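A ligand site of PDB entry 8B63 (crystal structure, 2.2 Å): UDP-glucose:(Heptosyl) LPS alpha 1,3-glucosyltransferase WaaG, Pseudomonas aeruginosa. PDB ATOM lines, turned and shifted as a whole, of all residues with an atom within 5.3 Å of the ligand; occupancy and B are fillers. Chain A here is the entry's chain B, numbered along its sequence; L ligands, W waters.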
ATOM      1  N   PRO A  13       2.436   1.103 -34.914  1.00  0.00           N
ATOM      2  CA  PRO A  13       1.494   2.212 -35.179  1.00  0.00           C
ATOM      3  C   PRO A  13       0.746   2.776 -33.971  1.00  0.00           C
ATOM      4  O   PRO A  13       0.227   3.898 -34.058  1.00  0.00           O
ATOM      5  CB  PRO A  13       0.443   1.587 -36.151  1.00  0.00           C
ATOM      6  CG  PRO A  13       1.159   0.394 -36.732  1.00  0.00           C
ATOM      7  CD  PRO A  13       2.006  -0.136 -35.592  1.00  0.00           C
ATOM      8  N   PHE A  14       0.658   2.030 -32.853  1.00  0.00           N
ATOM      9  CA  PHE A  14      -0.349   2.312 -31.834  1.00  0.00           C
ATOM     10  C   PHE A  14       0.282   2.792 -30.505  1.00  0.00           C
ATOM     11  O   PHE A  14      -0.187   2.457 -29.408  1.00  0.00           O
ATOM     12  CB  PHE A  14      -1.292   1.104 -31.714  1.00  0.00           C
ATOM     13  CG  PHE A  14      -1.992   0.667 -32.980  1.00  0.00           C
ATOM     14  CD1 PHE A  14      -2.424   1.600 -33.912  1.00  0.00           C
ATOM     15  CD2 PHE A  14      -2.170  -0.671 -33.278  1.00  0.00           C
ATOM     16  CE1 PHE A  14      -3.040   1.200 -35.093  1.00  0.00           C
ATOM     17  CE2 PHE A  14      -2.774  -1.078 -34.457  1.00  0.00           C
ATOM     18  CZ  PHE A  14      -3.225  -0.139 -35.358  1.00  0.00           C
ATOM     19  N   GLY A  15       1.304   3.654 -30.570  1.00  0.00           N
ATOM     20  CA  GLY A  15       1.915   4.240 -29.380  1.00  0.00           C
ATOM     21  C   GLY A  15       2.205   5.729 -29.577  1.00  0.00           C
ATOM     22  O   GLY A  15       2.400   6.165 -30.719  1.00  0.00           O
ATOM     23  N   GLY A  16       2.231   6.500 -28.468  1.00  0.00           N
ATOM     24  CA  GLY A  16       2.413   7.941 -28.509  1.00  0.00           C
ATOM     25  C   GLY A  16       3.774   8.359 -29.071  1.00  0.00           C
ATOM     26  O   GLY A  16       3.876   9.180 -29.996  1.00  0.00           O
ATOM     27  N   LEU A  17       4.843   7.783 -28.512  1.00  0.00           N
ATOM     28  CA  LEU A  17       6.208   7.989 -28.974  1.00  0.00           C
ATOM     29  C   LEU A  17       6.338   7.771 -30.479  1.00  0.00           C
ATOM     30  O   LEU A  17       6.923   8.573 -31.200  1.00  0.00           O
ATOM     31  CB  LEU A  17       7.116   7.012 -28.237  1.00  0.00           C
ATOM     32  CG  LEU A  17       8.620   7.153 -28.516  1.00  0.00           C
ATOM     33  CD1 LEU A  17       9.425   6.438 -27.408  1.00  0.00           C
ATOM     34  CD2 LEU A  17       8.989   6.611 -29.888  1.00  0.00           C
ATOM     35  N   ARG A  19       3.847   7.511 -32.909  1.00  0.00           N
ATOM     36  CA  ARG A  19       3.060   8.420 -33.770  1.00  0.00           C
ATOM     37  C   ARG A  19       3.694   9.813 -33.823  1.00  0.00           C
ATOM     38  O   ARG A  19       3.600  10.510 -34.835  1.00  0.00           O
ATOM     39  CB  ARG A  19       1.605   8.508 -33.285  1.00  0.00           C
ATOM     40  CG  ARG A  19       0.799   7.233 -33.515  1.00  0.00           C
ATOM     41  CD  ARG A  19      -0.583   7.202 -32.859  1.00  0.00           C
ATOM     42  NE  ARG A  19      -1.387   8.403 -33.106  1.00  0.00           N
ATOM     43  CZ  ARG A  19      -2.106   8.664 -34.200  1.00  0.00           C
ATOM     44  NH1 ARG A  19      -2.313   7.735 -35.112  1.00  0.00           N
ATOM     45  NH2 ARG A  19      -2.702   9.826 -34.329  1.00  0.00           N
ATOM     46  N   ARG A 174      -8.660  13.136 -35.168  1.00  0.00           N
ATOM     47  CA  ARG A 174      -9.250  12.884 -33.853  1.00  0.00           C
ATOM     48  C   ARG A 174     -10.326  13.931 -33.552  1.00  0.00           C
ATOM     49  O   ARG A 174     -11.101  13.736 -32.619  1.00  0.00           O
ATOM     50  CB  ARG A 174      -8.227  12.870 -32.714  1.00  0.00           C
ATOM     51  CG  ARG A 174      -7.727  11.476 -32.372  1.00  0.00           C
ATOM     52  CD  ARG A 174      -6.703  10.980 -33.371  1.00  0.00           C
ATOM     53  NE  ARG A 174      -6.093   9.744 -32.905  1.00  0.00           N
ATOM     54  CZ  ARG A 174      -5.852   8.675 -33.656  1.00  0.00           C
ATOM     55  NH1 ARG A 174      -6.272   8.655 -34.910  1.00  0.00           N
ATOM     56  NH2 ARG A 174      -5.230   7.642 -33.114  1.00  0.00           N
ATOM     57  N   ILE A 203      -7.976   3.757 -23.244  1.00  0.00           N
ATOM     58  CA  ILE A 203      -7.282   3.620 -24.514  1.00  0.00           C
ATOM     59  C   ILE A 203      -5.778   3.750 -24.293  1.00  0.00           C
ATOM     60  O   ILE A 203      -5.332   4.633 -23.572  1.00  0.00           O
ATOM     61  CB  ILE A 203      -7.823   4.640 -25.528  1.00  0.00           C
ATOM     62  CG1 ILE A 203      -9.272   4.298 -25.895  1.00  0.00           C
ATOM     63  CG2 ILE A 203      -6.934   4.708 -26.755  1.00  0.00           C
ATOM     64  CD1 ILE A 203      -9.976   5.421 -26.664  1.00  0.00           C
ATOM     65  N   GLY A 204      -5.018   2.890 -24.974  1.00  0.00           N
ATOM     66  CA  GLY A 204      -3.567   2.930 -25.012  1.00  0.00           C
ATOM     67  C   GLY A 204      -2.977   1.666 -24.385  1.00  0.00           C
ATOM     68  O   GLY A 204      -3.527   1.096 -23.415  1.00  0.00           O
ATOM     69  N   SER A 205      -1.849   1.237 -24.965  1.00  0.00           N
ATOM     70  CA  SER A 205      -1.119   0.104 -24.434  1.00  0.00           C
ATOM     71  C   SER A 205      -0.433   0.481 -23.107  1.00  0.00           C
ATOM     72  O   SER A 205      -0.113   1.649 -22.878  1.00  0.00           O
ATOM     73  CB  SER A 205      -0.153  -0.425 -25.467  1.00  0.00           C
ATOM     74  OG  SER A 205      -0.868  -0.973 -26.553  1.00  0.00           O
ATOM     75  N   LYS A 210      -1.466   2.480 -16.908  1.00  0.00           N
ATOM     76  CA  LYS A 210      -2.520   3.470 -17.144  1.00  0.00           C
ATOM     77  C   LYS A 210      -3.741   3.190 -16.267  1.00  0.00           C
ATOM     78  O   LYS A 210      -4.769   3.866 -16.409  1.00  0.00           O
ATOM     79  CB  LYS A 210      -2.829   3.495 -18.640  1.00  0.00           C
ATOM     80  CG  LYS A 210      -1.604   3.915 -19.429  1.00  0.00           C
ATOM     81  CD  LYS A 210      -1.712   3.871 -20.924  1.00  0.00           C
ATOM     82  CE  LYS A 210      -0.483   4.506 -21.548  1.00  0.00           C
ATOM     83  NZ  LYS A 210      -0.732   4.828 -22.958  1.00  0.00           N
ATOM     84  N   ILE A 235      -8.453  -0.682 -25.035  1.00  0.00           N
ATOM     85  CA  ILE A 235      -7.878  -0.849 -26.355  1.00  0.00           C
ATOM     86  C   ILE A 235      -6.366  -0.670 -26.302  1.00  0.00           C
ATOM     87  O   ILE A 235      -5.891   0.410 -25.968  1.00  0.00           O
ATOM     88  CB  ILE A 235      -8.536   0.109 -27.349  1.00  0.00           C
ATOM     89  CG1 ILE A 235     -10.057  -0.030 -27.299  1.00  0.00           C
ATOM     90  CG2 ILE A 235      -8.001  -0.122 -28.759  1.00  0.00           C
ATOM     91  CD1 ILE A 235     -10.785   1.053 -28.076  1.00  0.00           C
ATOM     92  N   GLY A 236      -5.619  -1.737 -26.616  1.00  0.00           N
ATOM     93  CA  GLY A 236      -4.161  -1.789 -26.440  1.00  0.00           C
ATOM     94  C   GLY A 236      -3.571  -3.160 -26.832  1.00  0.00           C
ATOM     95  O   GLY A 236      -4.287  -4.150 -26.904  1.00  0.00           O
ATOM     96  N   LYS A 260      -7.241  -5.582 -29.044  1.00  0.00           N
ATOM     97  CA  LYS A 260      -5.901  -5.265 -29.497  1.00  0.00           C
ATOM     98  C   LYS A 260      -5.910  -3.872 -30.114  1.00  0.00           C
ATOM     99  O   LYS A 260      -6.976  -3.344 -30.425  1.00  0.00           O
ATOM    100  CB  LYS A 260      -5.400  -6.280 -30.547  1.00  0.00           C
ATOM    101  CG  LYS A 260      -5.293  -7.715 -30.063  1.00  0.00           C
ATOM    102  CD  LYS A 260      -4.455  -7.831 -28.798  1.00  0.00           C
ATOM    103  CE  LYS A 260      -4.156  -9.269 -28.419  1.00  0.00           C
ATOM    104  NZ  LYS A 260      -3.105  -9.342 -27.370  1.00  0.00           N
ATOM    105  N   GLY A 261      -4.717  -3.314 -30.316  1.00  0.00           N
ATOM    106  CA  GLY A 261      -4.548  -2.011 -30.928  1.00  0.00           C
ATOM    107  C   GLY A 261      -5.273  -1.896 -32.263  1.00  0.00           C
ATOM    108  O   GLY A 261      -5.476  -2.901 -32.941  1.00  0.00           O
ATOM    109  N   ARG A 262      -5.672  -0.674 -32.645  1.00  0.00           N
ATOM    110  CA  ARG A 262      -6.422  -0.490 -33.881  1.00  0.00           C
ATOM    111  C   ARG A 262      -6.453   0.986 -34.268  1.00  0.00           C
ATOM    112  O   ARG A 262      -6.175   1.864 -33.459  1.00  0.00           O
ATOM    113  CB  ARG A 262      -7.826  -1.088 -33.767  1.00  0.00           C
ATOM    114  CG  ARG A 262      -8.561  -0.687 -32.490  1.00  0.00           C
ATOM    115  CD  ARG A 262      -9.804  -1.526 -32.275  1.00  0.00           C
ATOM    116  NE  ARG A 262     -10.741  -1.408 -33.392  1.00  0.00           N
ATOM    117  CZ  ARG A 262     -11.741  -2.251 -33.627  1.00  0.00           C
ATOM    118  NH1 ARG A 262     -11.857  -3.356 -32.908  1.00  0.00           N
ATOM    119  NH2 ARG A 262     -12.595  -2.001 -34.608  1.00  0.00           N
ATOM    120  N   SER A 263      -6.754   1.233 -35.545  1.00  0.00           N
ATOM    121  CA  SER A 263      -6.503   2.533 -36.156  1.00  0.00           C
ATOM    122  C   SER A 263      -7.758   3.403 -36.134  1.00  0.00           C
ATOM    123  O   SER A 263      -7.632   4.580 -36.453  1.00  0.00           O
ATOM    124  CB  SER A 263      -5.931   2.422 -37.546  1.00  0.00           C
ATOM    125  OG  SER A 263      -6.729   1.608 -38.369  1.00  0.00           O
ATOM    126  N   ILE A 265      -9.537   4.586 -33.532  1.00  0.00           N
ATOM    127  CA  ILE A 265      -9.723   5.157 -32.202  1.00  0.00           C
ATOM    128  C   ILE A 265     -10.758   6.292 -32.217  1.00  0.00           C
ATOM    129  O   ILE A 265     -11.540   6.428 -31.275  1.00  0.00           O
ATOM    130  CB  ILE A 265      -8.348   5.627 -31.670  1.00  0.00           C
ATOM    131  CG1 ILE A 265      -7.414   4.461 -31.376  1.00  0.00           C
ATOM    132  CG2 ILE A 265      -8.523   6.523 -30.459  1.00  0.00           C
ATOM    133  CD1 ILE A 265      -8.012   3.343 -30.533  1.00  0.00           C
ATOM    134  N   HIS A 277      -9.025   7.122 -17.285  1.00  0.00           N
ATOM    135  CA  HIS A 277      -7.587   7.013 -17.395  1.00  0.00           C
ATOM    136  C   HIS A 277      -6.925   7.237 -16.038  1.00  0.00           C
ATOM    137  O   HIS A 277      -6.152   8.158 -15.862  1.00  0.00           O
ATOM    138  CB  HIS A 277      -7.063   8.041 -18.421  1.00  0.00           C
ATOM    139  CG  HIS A 277      -5.677   7.798 -18.960  1.00  0.00           C
ATOM    140  ND1 HIS A 277      -5.451   7.001 -20.069  1.00  0.00           N
ATOM    141  CD2 HIS A 277      -4.466   8.267 -18.608  1.00  0.00           C
ATOM    142  CE1 HIS A 277      -4.145   6.986 -20.343  1.00  0.00           C
ATOM    143  NE2 HIS A 277      -3.532   7.746 -19.468  1.00  0.00           N
ATOM    144  N   GLU A 282       2.359   8.768 -16.103  1.00  0.00           N
ATOM    145  CA  GLU A 282       2.242   9.042 -17.521  1.00  0.00           C
ATOM    146  C   GLU A 282       2.940  10.367 -17.861  1.00  0.00           C
ATOM    147  O   GLU A 282       2.598  11.423 -17.353  1.00  0.00           O
ATOM    148  CB  GLU A 282       0.746   9.001 -17.864  1.00  0.00           C
ATOM    149  CG  GLU A 282       0.368   9.627 -19.189  1.00  0.00           C
ATOM    150  CD  GLU A 282      -0.010   8.666 -20.300  1.00  0.00           C
ATOM    151  OE1 GLU A 282       0.879   8.160 -20.990  1.00  0.00           O
ATOM    152  OE2 GLU A 282      -1.201   8.458 -20.469  1.00  0.00           O
ATOM    153  N   THR A 284       2.673  12.314 -20.522  1.00  0.00           N
ATOM    154  CA  THR A 284       1.694  13.290 -20.999  1.00  0.00           C
ATOM    155  C   THR A 284       0.290  12.664 -21.036  1.00  0.00           C
ATOM    156  O   THR A 284      -0.536  12.929 -20.159  1.00  0.00           O
ATOM    157  CB  THR A 284       2.044  13.880 -22.391  1.00  0.00           C
ATOM    158  OG1 THR A 284       2.369  12.845 -23.316  1.00  0.00           O
ATOM    159  CG2 THR A 284       3.223  14.835 -22.354  1.00  0.00           C
ATOM    160  N   GLY A 285       0.039  11.836 -22.064  1.00  0.00           N
ATOM    161  CA  GLY A 285      -1.262  11.200 -22.253  1.00  0.00           C
ATOM    162  C   GLY A 285      -2.007  11.816 -23.432  1.00  0.00           C
ATOM    163  O   GLY A 285      -3.006  12.468 -23.238  1.00  0.00           O
ATOM    164  N   THR A 286      -1.500  11.591 -24.656  1.00  0.00           N
ATOM    165  CA  THR A 286      -2.135  12.044 -25.892  1.00  0.00           C
ATOM    166  C   THR A 286      -3.639  11.758 -25.885  1.00  0.00           C
ATOM    167  O   THR A 286      -4.398  12.605 -26.297  1.00  0.00           O
ATOM    168  CB  THR A 286      -1.497  11.377 -27.122  1.00  0.00           C
ATOM    169  OG1 THR A 286      -0.072  11.549 -27.079  1.00  0.00           O
ATOM    170  CG2 THR A 286      -2.069  11.899 -28.425  1.00  0.00           C
ATOM    171  N   VAL A 287      -4.083  10.576 -25.443  1.00  0.00           N
ATOM    172  CA  VAL A 287      -5.491  10.196 -25.550  1.00  0.00           C
ATOM    173  C   VAL A 287      -6.380  11.144 -24.740  1.00  0.00           C
ATOM    174  O   VAL A 287      -7.529  11.336 -25.084  1.00  0.00           O
ATOM    175  CB  VAL A 287      -5.753   8.732 -25.129  1.00  0.00           C
ATOM    176  CG1 VAL A 287      -5.060   7.755 -26.077  1.00  0.00           C
ATOM    177  CG2 VAL A 287      -5.387   8.419 -23.682  1.00  0.00           C
ATOM    178  N   GLU A 290      -7.065  13.712 -27.084  1.00  0.00           N
ATOM    179  CA  GLU A 290      -7.832  13.141 -28.195  1.00  0.00           C
ATOM    180  C   GLU A 290      -9.322  13.012 -27.804  1.00  0.00           C
ATOM    181  O   GLU A 290     -10.208  13.317 -28.587  1.00  0.00           O
ATOM    182  CB  GLU A 290      -7.234  11.785 -28.587  1.00  0.00           C
ATOM    183  CG  GLU A 290      -5.909  11.864 -29.320  1.00  0.00           C
ATOM    184  CD  GLU A 290      -5.319  10.506 -29.717  1.00  0.00           C
ATOM    185  OE1 GLU A 290      -5.684   9.514 -29.050  1.00  0.00           O
ATOM    186  OE2 GLU A 290      -4.502  10.430 -30.697  1.00  0.00           O
HETATM  187  N1  LIG L   1      -3.523   4.541 -30.223  1.00  0.00           N
HETATM  188  C1  LIG L   1      -3.953   3.998 -31.436  1.00  0.00           C
HETATM  189  N2  LIG L   1      -4.490   2.736 -31.329  1.00  0.00           N
HETATM  190  C2  LIG L   1      -4.655   1.983 -30.178  1.00  0.00           C
HETATM  191  C3  LIG L   1      -4.184   2.602 -28.979  1.00  0.00           C
HETATM  192  C4  LIG L   1      -3.667   3.843 -29.046  1.00  0.00           C
HETATM  193  O1  LIG L   1      -3.872   4.594 -32.514  1.00  0.00           O
HETATM  194  O2  LIG L   1      -5.182   0.869 -30.235  1.00  0.00           O
HETATM  195  C5  LIG L   1      -2.935   5.888 -30.224  1.00  0.00           C
HETATM  196  C6  LIG L   1      -3.713   6.869 -29.353  1.00  0.00           C
HETATM  197  O3  LIG L   1      -4.892   7.261 -30.026  1.00  0.00           O
HETATM  198  C7  LIG L   1      -2.619   7.932 -29.166  1.00  0.00           C
HETATM  199  C8  LIG L   1      -1.372   7.068 -28.917  1.00  0.00           C
HETATM  200  O4  LIG L   1      -1.661   5.830 -29.636  1.00  0.00           O
HETATM  201  O5  LIG L   1      -2.458   8.707 -30.356  1.00  0.00           O
HETATM  202  C9  LIG L   1      -1.029   6.729 -27.483  1.00  0.00           C
HETATM  203  O6  LIG L   1      -0.385   7.882 -26.842  1.00  0.00           O
HETATM  204  P1  LIG L   1      -0.564   8.212 -25.289  1.00  0.00           P
HETATM  205  O7  LIG L   1       0.207   9.461 -24.992  1.00  0.00           O
HETATM  206  O8  LIG L   1      -2.022   8.179 -24.881  1.00  0.00           O
HETATM  207  O9  LIG L   1       0.074   6.940 -24.520  1.00  0.00           O
HETATM  208  P2  LIG L   1       1.500   6.208 -24.556  1.00  0.00           P
HETATM  209  O10 LIG L   1       2.461   7.322 -24.976  1.00  0.00           O
HETATM  210  O11 LIG L   1       1.648   5.677 -23.209  1.00  0.00           O
HETATM  211  O12 LIG L   1       1.434   5.089 -25.609  1.00  0.00           O
HETATM  212  O   HOH W   1      -1.042   3.443 -26.638  1.00  0.00           O
HETATM  213  O   HOH W   2      -2.974   6.156 -23.418  1.00  0.00           O
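N of Val 287 is in hydrogen-bond range of O8 of the ligand (3.2 Å).
O7 of the ligand is in hydrogen-bond range of OG1 of Thr 286, 3.0 Å away.
A nitrogen (N2) of the ligand lies within hydrogen-bond range of the backbone carbonyl oxygen (O) of Arg 262, 2.9 Å away.
N of Gly 16 sits at hydrogen-bond distance from O12 of the ligand (3.3 Å).
NZ of Lys 210 is in salt-bridge range of O11 of the ligand (2.5 Å).
The side-chain carboxylate of Glu 290 is in hydrogen-bond range of an oxygen (O3) of the ligand (2.6 Å).
An oxygen (O7) of the ligand is in hydrogen-bond range of the backbone NH (N) of Thr 286.
The guanidinium group (NE) of Arg 19 lies within hydrogen-bond range of an oxygen (O5) of the ligand (3.0 Å).
The backbone NH (N) of Arg 262 sits at hydrogen-bond distance from an oxygen (O2) of the ligand, 2.9 Å away.
An oxygen (O3) of the ligand lies within hydrogen-bond range of the guanidinium group of Arg 174.
The side-chain carboxylate of Glu 282 is in hydrogen-bond range of a ring nitrogen (NE2) of His 277 (2.6 Å).
NE of Arg 174 lies within salt-bridge range of OE2 of Glu 290 (2.8 Å).
The side-chain amino group of Lys 210 sits close to the backbone carbonyl oxygen of Ser 205, at 3.2 Å.
The backbone carbonyl oxygen (O) of Ile 235 sits at hydrogen-bond distance from the backbone NH (N) of Gly 204, at 2.8 Å.
The side-chain carboxylate (OE1) of Glu 282 lies close to an oxygen (O11) of the ligand (3.4 Å).
Residues that only touch the ligand: Phe 14 (3.5 Å), Gly 15 (3.8 Å), Ile 235 (3.3 Å), Gly 261 (3.0 Å), Ile 265 (3.4 Å) and Gly 285 (3.6 Å).
Water W2 lies within hydrogen-bond range of NZ of Lys 210 (2.6 Å), O8 of the ligand (2.7 Å) and O of Ile 203 (2.8 Å).
Water W1 lies within hydrogen-bond range of the backbone NH of Ser 205 (2.9 Å), the backbone carbonyl oxygen of Phe 14 (3.1 Å) and an oxygen (O12) of the ligand (3.1 Å).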
